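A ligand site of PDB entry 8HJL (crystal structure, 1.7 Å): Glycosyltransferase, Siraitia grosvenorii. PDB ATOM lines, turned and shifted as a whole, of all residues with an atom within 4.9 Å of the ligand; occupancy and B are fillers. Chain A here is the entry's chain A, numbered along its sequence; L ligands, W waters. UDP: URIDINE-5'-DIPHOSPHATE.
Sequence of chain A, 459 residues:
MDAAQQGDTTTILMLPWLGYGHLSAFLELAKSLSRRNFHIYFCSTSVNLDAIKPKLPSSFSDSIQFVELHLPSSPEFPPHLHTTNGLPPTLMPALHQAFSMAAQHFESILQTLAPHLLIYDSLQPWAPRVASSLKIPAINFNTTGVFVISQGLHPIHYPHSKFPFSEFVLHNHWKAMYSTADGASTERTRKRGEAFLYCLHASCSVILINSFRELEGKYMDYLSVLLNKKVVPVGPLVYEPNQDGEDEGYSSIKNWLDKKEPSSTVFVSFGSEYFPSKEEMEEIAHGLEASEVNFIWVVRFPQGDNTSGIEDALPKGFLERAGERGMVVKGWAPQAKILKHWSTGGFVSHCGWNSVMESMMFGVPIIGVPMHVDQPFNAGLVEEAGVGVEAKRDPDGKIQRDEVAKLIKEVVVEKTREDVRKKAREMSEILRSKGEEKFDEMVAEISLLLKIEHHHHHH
The indole nitrogen (NE1) of Trp 332 sits close to a nitrogen (N3) of the ligand, 3.4 Å away.
The backbone carbonyl oxygen of Gly 352 lies close to an oxygen (O2A) of the ligand, 3.4 Å away.
Merely in contact with the ligand: Tyr 20 (3.3 Å), Ser 269 (3.5 Å), Val 298 (3.6 Å), Lys 55 (3.7 Å), Gly 271 (3.7 Å), Gly 21 (3.8 Å) and Glu 273 (3.8 Å).
Hydrophobic or aromatic side chains that line the ligand: Tyr 20, Val 298, Trp 332 and His 350.
Within 4 Å of the ligand: Tyr 20, Gly 21, Lys 55, Ser 269, Gly 271, Ser 272, Glu 273, Val 298, Trp 332, Ala 333, Gln 335, His 350, Gly 352, Trp 353, Asn 354, Ser 355 and Glu 358.
The nearest printed residue that does not touch the ligand is Gln 375 (4.2 Å).
ND1 of His 350 sits close to N of Gly 352 (3.4 Å).
The side-chain hydroxyl (OG) of Ser 355 lies within hydrogen-bond range of the side-chain amide nitrogen (NE2) of Gln 335.
The side-chain amino group (NZ) of Lys 55 lies within hydrogen-bond range of the side-chain hydroxyl (OG) of Ser 24, 3.3 Å away.
The backbone carbonyl oxygen (O) of Tyr 20 lies within hydrogen-bond range of the side-chain hydroxyl (OG) of Ser 24 (2.9 Å).
N of Gly 271 sits at hydrogen-bond distance from OG of Ser 269, at 3.3 Å.
N of His 350 sits at hydrogen-bond distance from O of Ser 269 (3.4 Å).
O of Gly 21 lies within hydrogen-bond range of ND2 of Asn 354 (2.9 Å).
NE2 of Gln 335 lies within hydrogen-bond range of OE1 of Glu 358, 3.1 Å away.
ND2 of Asn 354 sits at hydrogen-bond distance from O1A of the ligand, 2.9 Å away.
O3B of the ligand is in hydrogen-bond range of NE2 of His 350 (2.9 Å).
OG of Ser 355 sits at hydrogen-bond distance from O2A of the ligand.
The side-chain carboxylate of Glu 358 is in hydrogen-bond range of an oxygen (O3') of the ligand (2.7 Å).
An oxygen (O1B) of the ligand is in hydrogen-bond range of the backbone NH of Ser 272.
O of Ala 333 is in hydrogen-bond range of N3 of the ligand (2.6 Å).
The backbone NH (N) of Ala 333 sits at hydrogen-bond distance from an oxygen (O4) of the ligand (3.0 Å).
N of Asn 354 lies within hydrogen-bond range of O1A of the ligand (3.0 Å).
The side-chain amide nitrogen (NE2) of Gln 335 sits close to an oxygen (O2') of the ligand.
The backbone NH (N) of Trp 353 sits at hydrogen-bond distance from an oxygen (O1A) of the ligand (3.3 Å).
OG of Ser 272 lies within hydrogen-bond range of O1B of the ligand (2.6 Å).
An oxygen (O2A) of the ligand is in hydrogen-bond range of the backbone NH of Ser 355.
Water W8 bridges O2B of the ligand (2.6 Å) and N of Gly 21 (2.8 Å).
Water W6 lies within hydrogen-bond range of O3B of the ligand, NE2 of Gln 375 and OE2 of Glu 273.
Water W4 lies within hydrogen-bond range of an oxygen (O3B) of the ligand (2.7 Å), the backbone carbonyl oxygen of Phe 270 (2.8 Å), the backbone NH of Glu 273 (2.9 Å), the backbone NH of Ser 272 (3.3 Å) and a ring nitrogen (NE2) of His 350 (3.5 Å).
Water W2 bridges an oxygen (O2') of the ligand (2.8 Å) and the side-chain amino group (NZ) of Lys 55 (3.3 Å).
Water W3 lies within hydrogen-bond range of the backbone NH of Gln 335 (3.3 Å) and an oxygen (O2) of the ligand (3.4 Å).
Water W5 lies within hydrogen-bond range of OG of Ser 269 (2.6 Å), OE1 of Gln 335 (2.7 Å), OG of Ser 355 (3.2 Å) and N of Gly 271 (3.3 Å).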
ATOM      1  N   TYR A  20     -27.250  -7.268   8.570  1.00  0.00           N
ATOM      2  CA  TYR A  20     -26.015  -6.588   8.169  1.00  0.00           C
ATOM      3  C   TYR A  20     -26.284  -5.138   7.741  1.00  0.00           C
ATOM      4  O   TYR A  20     -25.513  -4.242   8.094  1.00  0.00           O
ATOM      5  CB  TYR A  20     -25.316  -7.361   7.064  1.00  0.00           C
ATOM      6  CG  TYR A  20     -24.006  -6.739   6.703  1.00  0.00           C
ATOM      7  CD1 TYR A  20     -22.851  -7.053   7.414  1.00  0.00           C
ATOM      8  CD2 TYR A  20     -23.921  -5.819   5.668  1.00  0.00           C
ATOM      9  CE1 TYR A  20     -21.637  -6.474   7.085  1.00  0.00           C
ATOM     10  CE2 TYR A  20     -22.725  -5.227   5.339  1.00  0.00           C
ATOM     11  CZ  TYR A  20     -21.583  -5.559   6.053  1.00  0.00           C
ATOM     12  OH  TYR A  20     -20.388  -4.968   5.714  1.00  0.00           O
ATOM     13  N   GLY A  21     -27.364  -4.911   6.981  1.00  0.00           N
ATOM     14  CA  GLY A  21     -27.687  -3.552   6.575  1.00  0.00           C
ATOM     15  C   GLY A  21     -27.965  -2.642   7.746  1.00  0.00           C
ATOM     16  O   GLY A  21     -27.619  -1.446   7.723  1.00  0.00           O
ATOM     17  N   SER A  24     -24.741  -1.965   9.664  1.00  0.00           N
ATOM     18  CA  SER A  24     -23.988  -1.011   8.845  1.00  0.00           C
ATOM     19  C   SER A  24     -24.428   0.421   9.096  1.00  0.00           C
ATOM     20  O   SER A  24     -23.597   1.314   9.304  1.00  0.00           O
ATOM     21  CB  SER A  24     -24.141  -1.360   7.357  1.00  0.00           C
ATOM     22  OG  SER A  24     -23.400  -2.511   7.007  1.00  0.00           O
ATOM     23  N   LYS A  55     -15.293  -2.722   9.238  1.00  0.00           N
ATOM     24  CA  LYS A  55     -15.708  -1.378   8.851  1.00  0.00           C
ATOM     25  C   LYS A  55     -15.455  -0.342   9.937  1.00  0.00           C
ATOM     26  O   LYS A  55     -15.814   0.821   9.753  1.00  0.00           O
ATOM     27  CB  LYS A  55     -17.203  -1.376   8.476  1.00  0.00           C
ATOM     28  CG  LYS A  55     -17.511  -1.908   7.067  1.00  0.00           C
ATOM     29  CD  LYS A  55     -19.010  -1.836   6.778  1.00  0.00           C
ATOM     30  CE  LYS A  55     -19.337  -2.076   5.315  1.00  0.00           C
ATOM     31  NZ  LYS A  55     -20.809  -1.904   5.045  1.00  0.00           N
ATOM     32  N   PHE A 267     -22.285  -3.636 -11.513  1.00  0.00           N
ATOM     33  CA  PHE A 267     -22.247  -4.478 -10.334  1.00  0.00           C
ATOM     34  C   PHE A 267     -23.658  -5.031 -10.132  1.00  0.00           C
ATOM     35  O   PHE A 267     -24.641  -4.331 -10.387  1.00  0.00           O
ATOM     36  CB  PHE A 267     -21.815  -3.658  -9.111  1.00  0.00           C
ATOM     37  CG  PHE A 267     -21.616  -4.477  -7.857  1.00  0.00           C
ATOM     38  CD1 PHE A 267     -20.737  -5.542  -7.853  1.00  0.00           C
ATOM     39  CD2 PHE A 267     -22.301  -4.157  -6.692  1.00  0.00           C
ATOM     40  CE1 PHE A 267     -20.535  -6.300  -6.705  1.00  0.00           C
ATOM     41  CE2 PHE A 267     -22.119  -4.912  -5.542  1.00  0.00           C
ATOM     42  CZ  PHE A 267     -21.252  -5.987  -5.557  1.00  0.00           C
ATOM     43  N   SER A 269     -26.012  -7.160  -7.299  1.00  0.00           N
ATOM     44  CA  SER A 269     -26.045  -7.690  -5.941  1.00  0.00           C
ATOM     45  C   SER A 269     -27.456  -7.607  -5.382  1.00  0.00           C
ATOM     46  O   SER A 269     -28.187  -6.652  -5.650  1.00  0.00           O
ATOM     47  CB  SER A 269     -25.064  -6.922  -5.029  1.00  0.00           C
ATOM     48  OG  SER A 269     -25.208  -7.323  -3.663  1.00  0.00           O
ATOM     49  N   PHE A 270     -27.821  -8.601  -4.580  1.00  0.00           N
ATOM     50  CA  PHE A 270     -29.133  -8.574  -3.934  1.00  0.00           C
ATOM     51  C   PHE A 270     -29.008  -8.482  -2.422  1.00  0.00           C
ATOM     52  O   PHE A 270     -29.864  -8.952  -1.687  1.00  0.00           O
ATOM     53  CB  PHE A 270     -29.995  -9.744  -4.417  1.00  0.00           C
ATOM     54  CG  PHE A 270     -30.230  -9.714  -5.891  1.00  0.00           C
ATOM     55  CD1 PHE A 270     -31.291  -9.001  -6.433  1.00  0.00           C
ATOM     56  CD2 PHE A 270     -29.308 -10.264  -6.762  1.00  0.00           C
ATOM     57  CE1 PHE A 270     -31.470  -8.918  -7.796  1.00  0.00           C
ATOM     58  CE2 PHE A 270     -29.479 -10.192  -8.124  1.00  0.00           C
ATOM     59  CZ  PHE A 270     -30.552  -9.505  -8.643  1.00  0.00           C
ATOM     60  N   GLY A 271     -27.944  -7.832  -1.960  1.00  0.00           N
ATOM     61  CA  GLY A 271     -27.813  -7.528  -0.547  1.00  0.00           C
ATOM     62  C   GLY A 271     -27.367  -8.730   0.279  1.00  0.00           C
ATOM     63  O   GLY A 271     -26.814  -9.726  -0.221  1.00  0.00           O
ATOM     64  N   SER A 272     -27.662  -8.638   1.573  1.00  0.00           N
ATOM     65  CA  SER A 272     -27.160  -9.602   2.535  1.00  0.00           C
ATOM     66  C   SER A 272     -28.191 -10.623   2.989  1.00  0.00           C
ATOM     67  O   SER A 272     -27.801 -11.590   3.647  1.00  0.00           O
ATOM     68  CB  SER A 272     -26.620  -8.877   3.787  1.00  0.00           C
ATOM     69  OG  SER A 272     -27.682  -8.259   4.522  1.00  0.00           O
ATOM     70  N   GLU A 273     -29.475 -10.463   2.675  1.00  0.00           N
ATOM     71  CA  GLU A 273     -30.451 -11.369   3.235  1.00  0.00           C
ATOM     72  C   GLU A 273     -31.509 -11.732   2.204  1.00  0.00           C
ATOM     73  O   GLU A 273     -32.708 -11.738   2.491  1.00  0.00           O
ATOM     74  CB  GLU A 273     -31.090 -10.802   4.505  1.00  0.00           C
ATOM     75  CG  GLU A 273     -31.252  -9.302   4.527  1.00  0.00           C
ATOM     76  CD  GLU A 273     -32.228  -8.805   5.608  1.00  0.00           C
ATOM     77  OE1 GLU A 273     -32.410  -9.490   6.620  1.00  0.00           O
ATOM     78  OE2 GLU A 273     -32.825  -7.730   5.410  1.00  0.00           O
ATOM     79  N   VAL A 298     -22.450 -10.861  -7.610  1.00  0.00           N
ATOM     80  CA  VAL A 298     -22.289 -11.548  -6.323  1.00  0.00           C
ATOM     81  C   VAL A 298     -23.385 -12.583  -6.215  1.00  0.00           C
ATOM     82  O   VAL A 298     -24.571 -12.246  -6.231  1.00  0.00           O
ATOM     83  CB  VAL A 298     -22.353 -10.577  -5.135  1.00  0.00           C
ATOM     84  CG1 VAL A 298     -22.163 -11.347  -3.824  1.00  0.00           C
ATOM     85  CG2 VAL A 298     -21.329  -9.481  -5.253  1.00  0.00           C
ATOM     86  N   GLY A 331     -20.251 -15.306  -2.570  1.00  0.00           N
ATOM     87  CA  GLY A 331     -20.422 -14.987  -1.154  1.00  0.00           C
ATOM     88  C   GLY A 331     -20.494 -13.518  -0.795  1.00  0.00           C
ATOM     89  O   GLY A 331     -21.440 -13.097  -0.132  1.00  0.00           O
ATOM     90  N   TRP A 332     -19.509 -12.733  -1.235  1.00  0.00           N
ATOM     91  CA  TRP A 332     -19.358 -11.360  -0.794  1.00  0.00           C
ATOM     92  C   TRP A 332     -18.322 -10.656  -1.664  1.00  0.00           C
ATOM     93  O   TRP A 332     -17.352 -11.271  -2.100  1.00  0.00           O
ATOM     94  CB  TRP A 332     -18.915 -11.289   0.675  1.00  0.00           C
ATOM     95  CG  TRP A 332     -19.236  -9.994   1.362  1.00  0.00           C
ATOM     96  CD1 TRP A 332     -18.370  -8.977   1.646  1.00  0.00           C
ATOM     97  CD2 TRP A 332     -20.530  -9.581   1.842  1.00  0.00           C
ATOM     98  NE1 TRP A 332     -19.041  -7.959   2.295  1.00  0.00           N
ATOM     99  CE2 TRP A 332     -20.363  -8.298   2.421  1.00  0.00           C
ATOM    100  CE3 TRP A 332     -21.796 -10.164   1.853  1.00  0.00           C
ATOM    101  CZ2 TRP A 332     -21.423  -7.595   2.997  1.00  0.00           C
ATOM    102  CZ3 TRP A 332     -22.855  -9.452   2.419  1.00  0.00           C
ATOM    103  CH2 TRP A 332     -22.662  -8.185   2.977  1.00  0.00           C
ATOM    104  N   ALA A 333     -18.531  -9.366  -1.871  1.00  0.00           N
ATOM    105  CA  ALA A 333     -17.686  -8.529  -2.708  1.00  0.00           C
ATOM    106  C   ALA A 333     -17.513  -7.178  -2.045  1.00  0.00           C
ATOM    107  O   ALA A 333     -18.399  -6.737  -1.288  1.00  0.00           O
ATOM    108  CB  ALA A 333     -18.256  -8.340  -4.109  1.00  0.00           C
ATOM    109  N   PRO A 334     -16.399  -6.487  -2.316  1.00  0.00           N
ATOM    110  CA  PRO A 334     -16.224  -5.121  -1.806  1.00  0.00           C
ATOM    111  C   PRO A 334     -17.094  -4.132  -2.558  1.00  0.00           C
ATOM    112  O   PRO A 334     -16.638  -3.471  -3.499  1.00  0.00           O
ATOM    113  CB  PRO A 334     -14.727  -4.857  -2.019  1.00  0.00           C
ATOM    114  CG  PRO A 334     -14.324  -5.786  -3.097  1.00  0.00           C
ATOM    115  CD  PRO A 334     -15.174  -7.016  -2.941  1.00  0.00           C
ATOM    116  N   GLN A 335     -18.362  -4.045  -2.153  1.00  0.00           N
ATOM    117  CA  GLN A 335     -19.345  -3.307  -2.945  1.00  0.00           C
ATOM    118  C   GLN A 335     -18.939  -1.845  -3.156  1.00  0.00           C
ATOM    119  O   GLN A 335     -18.976  -1.343  -4.285  1.00  0.00           O
ATOM    120  CB  GLN A 335     -20.723  -3.391  -2.273  1.00  0.00           C
ATOM    121  CG  GLN A 335     -21.760  -2.434  -2.879  1.00  0.00           C
ATOM    122  CD  GLN A 335     -23.216  -2.858  -2.584  1.00  0.00           C
ATOM    123  OE1 GLN A 335     -23.525  -4.049  -2.455  1.00  0.00           O
ATOM    124  NE2 GLN A 335     -24.093  -1.877  -2.510  1.00  0.00           N
ATOM    125  N   HIS A 350     -31.039  -4.865  -5.740  1.00  0.00           N
ATOM    126  CA  HIS A 350     -32.309  -5.159  -5.089  1.00  0.00           C
ATOM    127  C   HIS A 350     -32.895  -3.937  -4.405  1.00  0.00           C
ATOM    128  O   HIS A 350     -34.010  -4.024  -3.885  1.00  0.00           O
ATOM    129  CB  HIS A 350     -32.175  -6.296  -4.063  1.00  0.00           C
ATOM    130  CG  HIS A 350     -31.557  -5.881  -2.759  1.00  0.00           C
ATOM    131  ND1 HIS A 350     -30.377  -5.175  -2.674  1.00  0.00           N
ATOM    132  CD2 HIS A 350     -31.944  -6.111  -1.470  1.00  0.00           C
ATOM    133  CE1 HIS A 350     -30.053  -4.996  -1.417  1.00  0.00           C
ATOM    134  NE2 HIS A 350     -30.990  -5.542  -0.659  1.00  0.00           N
ATOM    135  N   GLY A 352     -32.015  -2.388  -1.631  1.00  0.00           N
ATOM    136  CA  GLY A 352     -31.842  -2.141  -0.216  1.00  0.00           C
ATOM    137  C   GLY A 352     -31.287  -0.749  -0.001  1.00  0.00           C
ATOM    138  O   GLY A 352     -30.571  -0.219  -0.850  1.00  0.00           O
ATOM    139  N   TRP A 353     -31.644  -0.135   1.132  1.00  0.00           N
ATOM    140  CA  TRP A 353     -31.482   1.316   1.253  1.00  0.00           C
ATOM    141  C   TRP A 353     -30.021   1.721   1.382  1.00  0.00           C
ATOM    142  O   TRP A 353     -29.610   2.765   0.855  1.00  0.00           O
ATOM    143  CB  TRP A 353     -32.307   1.831   2.441  1.00  0.00           C
ATOM    144  CG  TRP A 353     -32.357   3.316   2.486  1.00  0.00           C
ATOM    145  CD1 TRP A 353     -31.790   4.141   3.445  1.00  0.00           C
ATOM    146  CD2 TRP A 353     -32.976   4.177   1.533  1.00  0.00           C
ATOM    147  NE1 TRP A 353     -32.044   5.447   3.129  1.00  0.00           N
ATOM    148  CE2 TRP A 353     -32.770   5.511   1.973  1.00  0.00           C
ATOM    149  CE3 TRP A 353     -33.696   3.962   0.350  1.00  0.00           C
ATOM    150  CZ2 TRP A 353     -33.254   6.611   1.280  1.00  0.00           C
ATOM    151  CZ3 TRP A 353     -34.189   5.065  -0.332  1.00  0.00           C
ATOM    152  CH2 TRP A 353     -33.964   6.378   0.129  1.00  0.00           C
ATOM    153  N   ASN A 354     -29.206   0.927   2.072  1.00  0.00           N
ATOM    154  CA  ASN A 354     -27.795   1.257   2.091  1.00  0.00           C
ATOM    155  C   ASN A 354     -27.205   1.212   0.689  1.00  0.00           C
ATOM    156  O   ASN A 354     -26.424   2.094   0.307  1.00  0.00           O
ATOM    157  CB  ASN A 354     -27.015   0.331   3.027  1.00  0.00           C
ATOM    158  CG  ASN A 354     -27.478   0.453   4.473  1.00  0.00           C
ATOM    159  OD1 ASN A 354     -27.217   1.456   5.139  1.00  0.00           O
ATOM    160  ND2 ASN A 354     -28.145  -0.588   4.961  1.00  0.00           N
ATOM    161  N   SER A 355     -27.614   0.227  -0.118  1.00  0.00           N
ATOM    162  CA  SER A 355     -27.088   0.145  -1.482  1.00  0.00           C
ATOM    163  C   SER A 355     -27.558   1.330  -2.315  1.00  0.00           C
ATOM    164  O   SER A 355     -26.817   1.826  -3.163  1.00  0.00           O
ATOM    165  CB  SER A 355     -27.509  -1.178  -2.128  1.00  0.00           C
ATOM    166  OG  SER A 355     -26.884  -2.271  -1.457  1.00  0.00           O
ATOM    167  N   GLU A 358     -25.466   4.396  -1.050  1.00  0.00           N
ATOM    168  CA  GLU A 358     -24.112   4.281  -1.612  1.00  0.00           C
ATOM    169  C   GLU A 358     -24.083   4.637  -3.085  1.00  0.00           C
ATOM    170  O   GLU A 358     -23.204   5.396  -3.535  1.00  0.00           O
ATOM    171  CB  GLU A 358     -23.599   2.846  -1.385  1.00  0.00           C
ATOM    172  CG  GLU A 358     -23.238   2.593   0.079  1.00  0.00           C
ATOM    173  CD  GLU A 358     -23.268   1.114   0.483  1.00  0.00           C
ATOM    174  OE1 GLU A 358     -23.373   0.220  -0.386  1.00  0.00           O
ATOM    175  OE2 GLU A 358     -23.177   0.856   1.697  1.00  0.00           O
ATOM    176  N   GLN A 375     -37.822  -2.691  -0.395  1.00  0.00           N
ATOM    177  CA  GLN A 375     -37.137  -2.505  -1.675  1.00  0.00           C
ATOM    178  C   GLN A 375     -38.027  -2.000  -2.826  1.00  0.00           C
ATOM    179  O   GLN A 375     -37.549  -1.141  -3.585  1.00  0.00           O
ATOM    180  CB  GLN A 375     -36.465  -3.830  -2.045  1.00  0.00           C
ATOM    181  CG  GLN A 375     -35.431  -4.206  -1.016  1.00  0.00           C
ATOM    182  CD  GLN A 375     -35.190  -5.688  -0.945  1.00  0.00           C
ATOM    183  OE1 GLN A 375     -35.468  -6.413  -1.907  1.00  0.00           O
ATOM    184  NE2 GLN A 375     -34.671  -6.160   0.183  1.00  0.00           N
HETATM  185  N1  UDP L   1     -22.676  -5.431   0.731  1.00  0.00           N
HETATM  186  C2  UDP L   1     -21.232  -5.621   0.471  1.00  0.00           C
HETATM  187  N3  UDP L   1     -20.826  -6.753  -0.388  1.00  0.00           N
HETATM  188  C4  UDP L   1     -21.804  -7.641  -0.976  1.00  0.00           C
HETATM  189  C5  UDP L   1     -23.247  -7.442  -0.718  1.00  0.00           C
HETATM  190  C6  UDP L   1     -23.674  -6.316   0.154  1.00  0.00           C
HETATM  191  O2  UDP L   1     -20.437  -4.888   0.958  1.00  0.00           O
HETATM  192  O4  UDP L   1     -21.431  -8.530  -1.683  1.00  0.00           O
HETATM  193  C1' UDP L   1     -23.066  -4.330   1.612  1.00  0.00           C
HETATM  194  C2' UDP L   1     -23.618  -3.108   0.813  1.00  0.00           C
HETATM  195  O2' UDP L   1     -22.589  -2.271   0.456  1.00  0.00           O
HETATM  196  C3' UDP L   1     -24.529  -2.493   1.859  1.00  0.00           C
HETATM  197  C4' UDP L   1     -25.006  -3.535   2.613  1.00  0.00           C
HETATM  198  O4' UDP L   1     -24.015  -4.762   2.380  1.00  0.00           O
HETATM  199  O3' UDP L   1     -23.667  -1.628   2.741  1.00  0.00           O
HETATM  200  C5' UDP L   1     -26.328  -4.076   2.142  1.00  0.00           C
HETATM  201  O5' UDP L   1     -27.317  -3.346   2.791  1.00  0.00           O
HETATM  202  PA  UDP L   1     -28.662  -3.018   1.933  1.00  0.00           P
HETATM  203  O1A UDP L   1     -29.447  -2.027   2.754  1.00  0.00           O
HETATM  204  O2A UDP L   1     -28.400  -2.505   0.548  1.00  0.00           O
HETATM  205  O3A UDP L   1     -29.627  -4.332   1.784  1.00  0.00           O
HETATM  206  PB  UDP L   1     -29.825  -5.591   2.817  1.00  0.00           P
HETATM  207  O1B UDP L   1     -28.580  -6.445   2.944  1.00  0.00           O
HETATM  208  O2B UDP L   1     -30.221  -5.062   4.171  1.00  0.00           O
HETATM  209  O3B UDP L   1     -30.978  -6.277   2.174  1.00  0.00           O
HETATM  210  O   HOH W   1     -17.548  -4.888   1.704  1.00  0.00           O
HETATM  211  O   HOH W   2     -20.290  -1.423   1.788  1.00  0.00           O
HETATM  212  O   HOH W   3     -18.242  -2.326   0.687  1.00  0.00           O
HETATM  213  O   HOH W   4     -30.924  -8.656   0.909  1.00  0.00           O
HETATM  214  O   HOH W   5     -25.896  -5.263  -2.178  1.00  0.00           O
HETATM  215  O   HOH W   6     -33.538  -6.052   2.953  1.00  0.00           O
HETATM  216  O   HOH W   7     -25.111  -9.838  -2.261  1.00  0.00           O
HETATM  217  O   HOH W   8     -29.874  -6.126   6.544  1.00  0.00           O
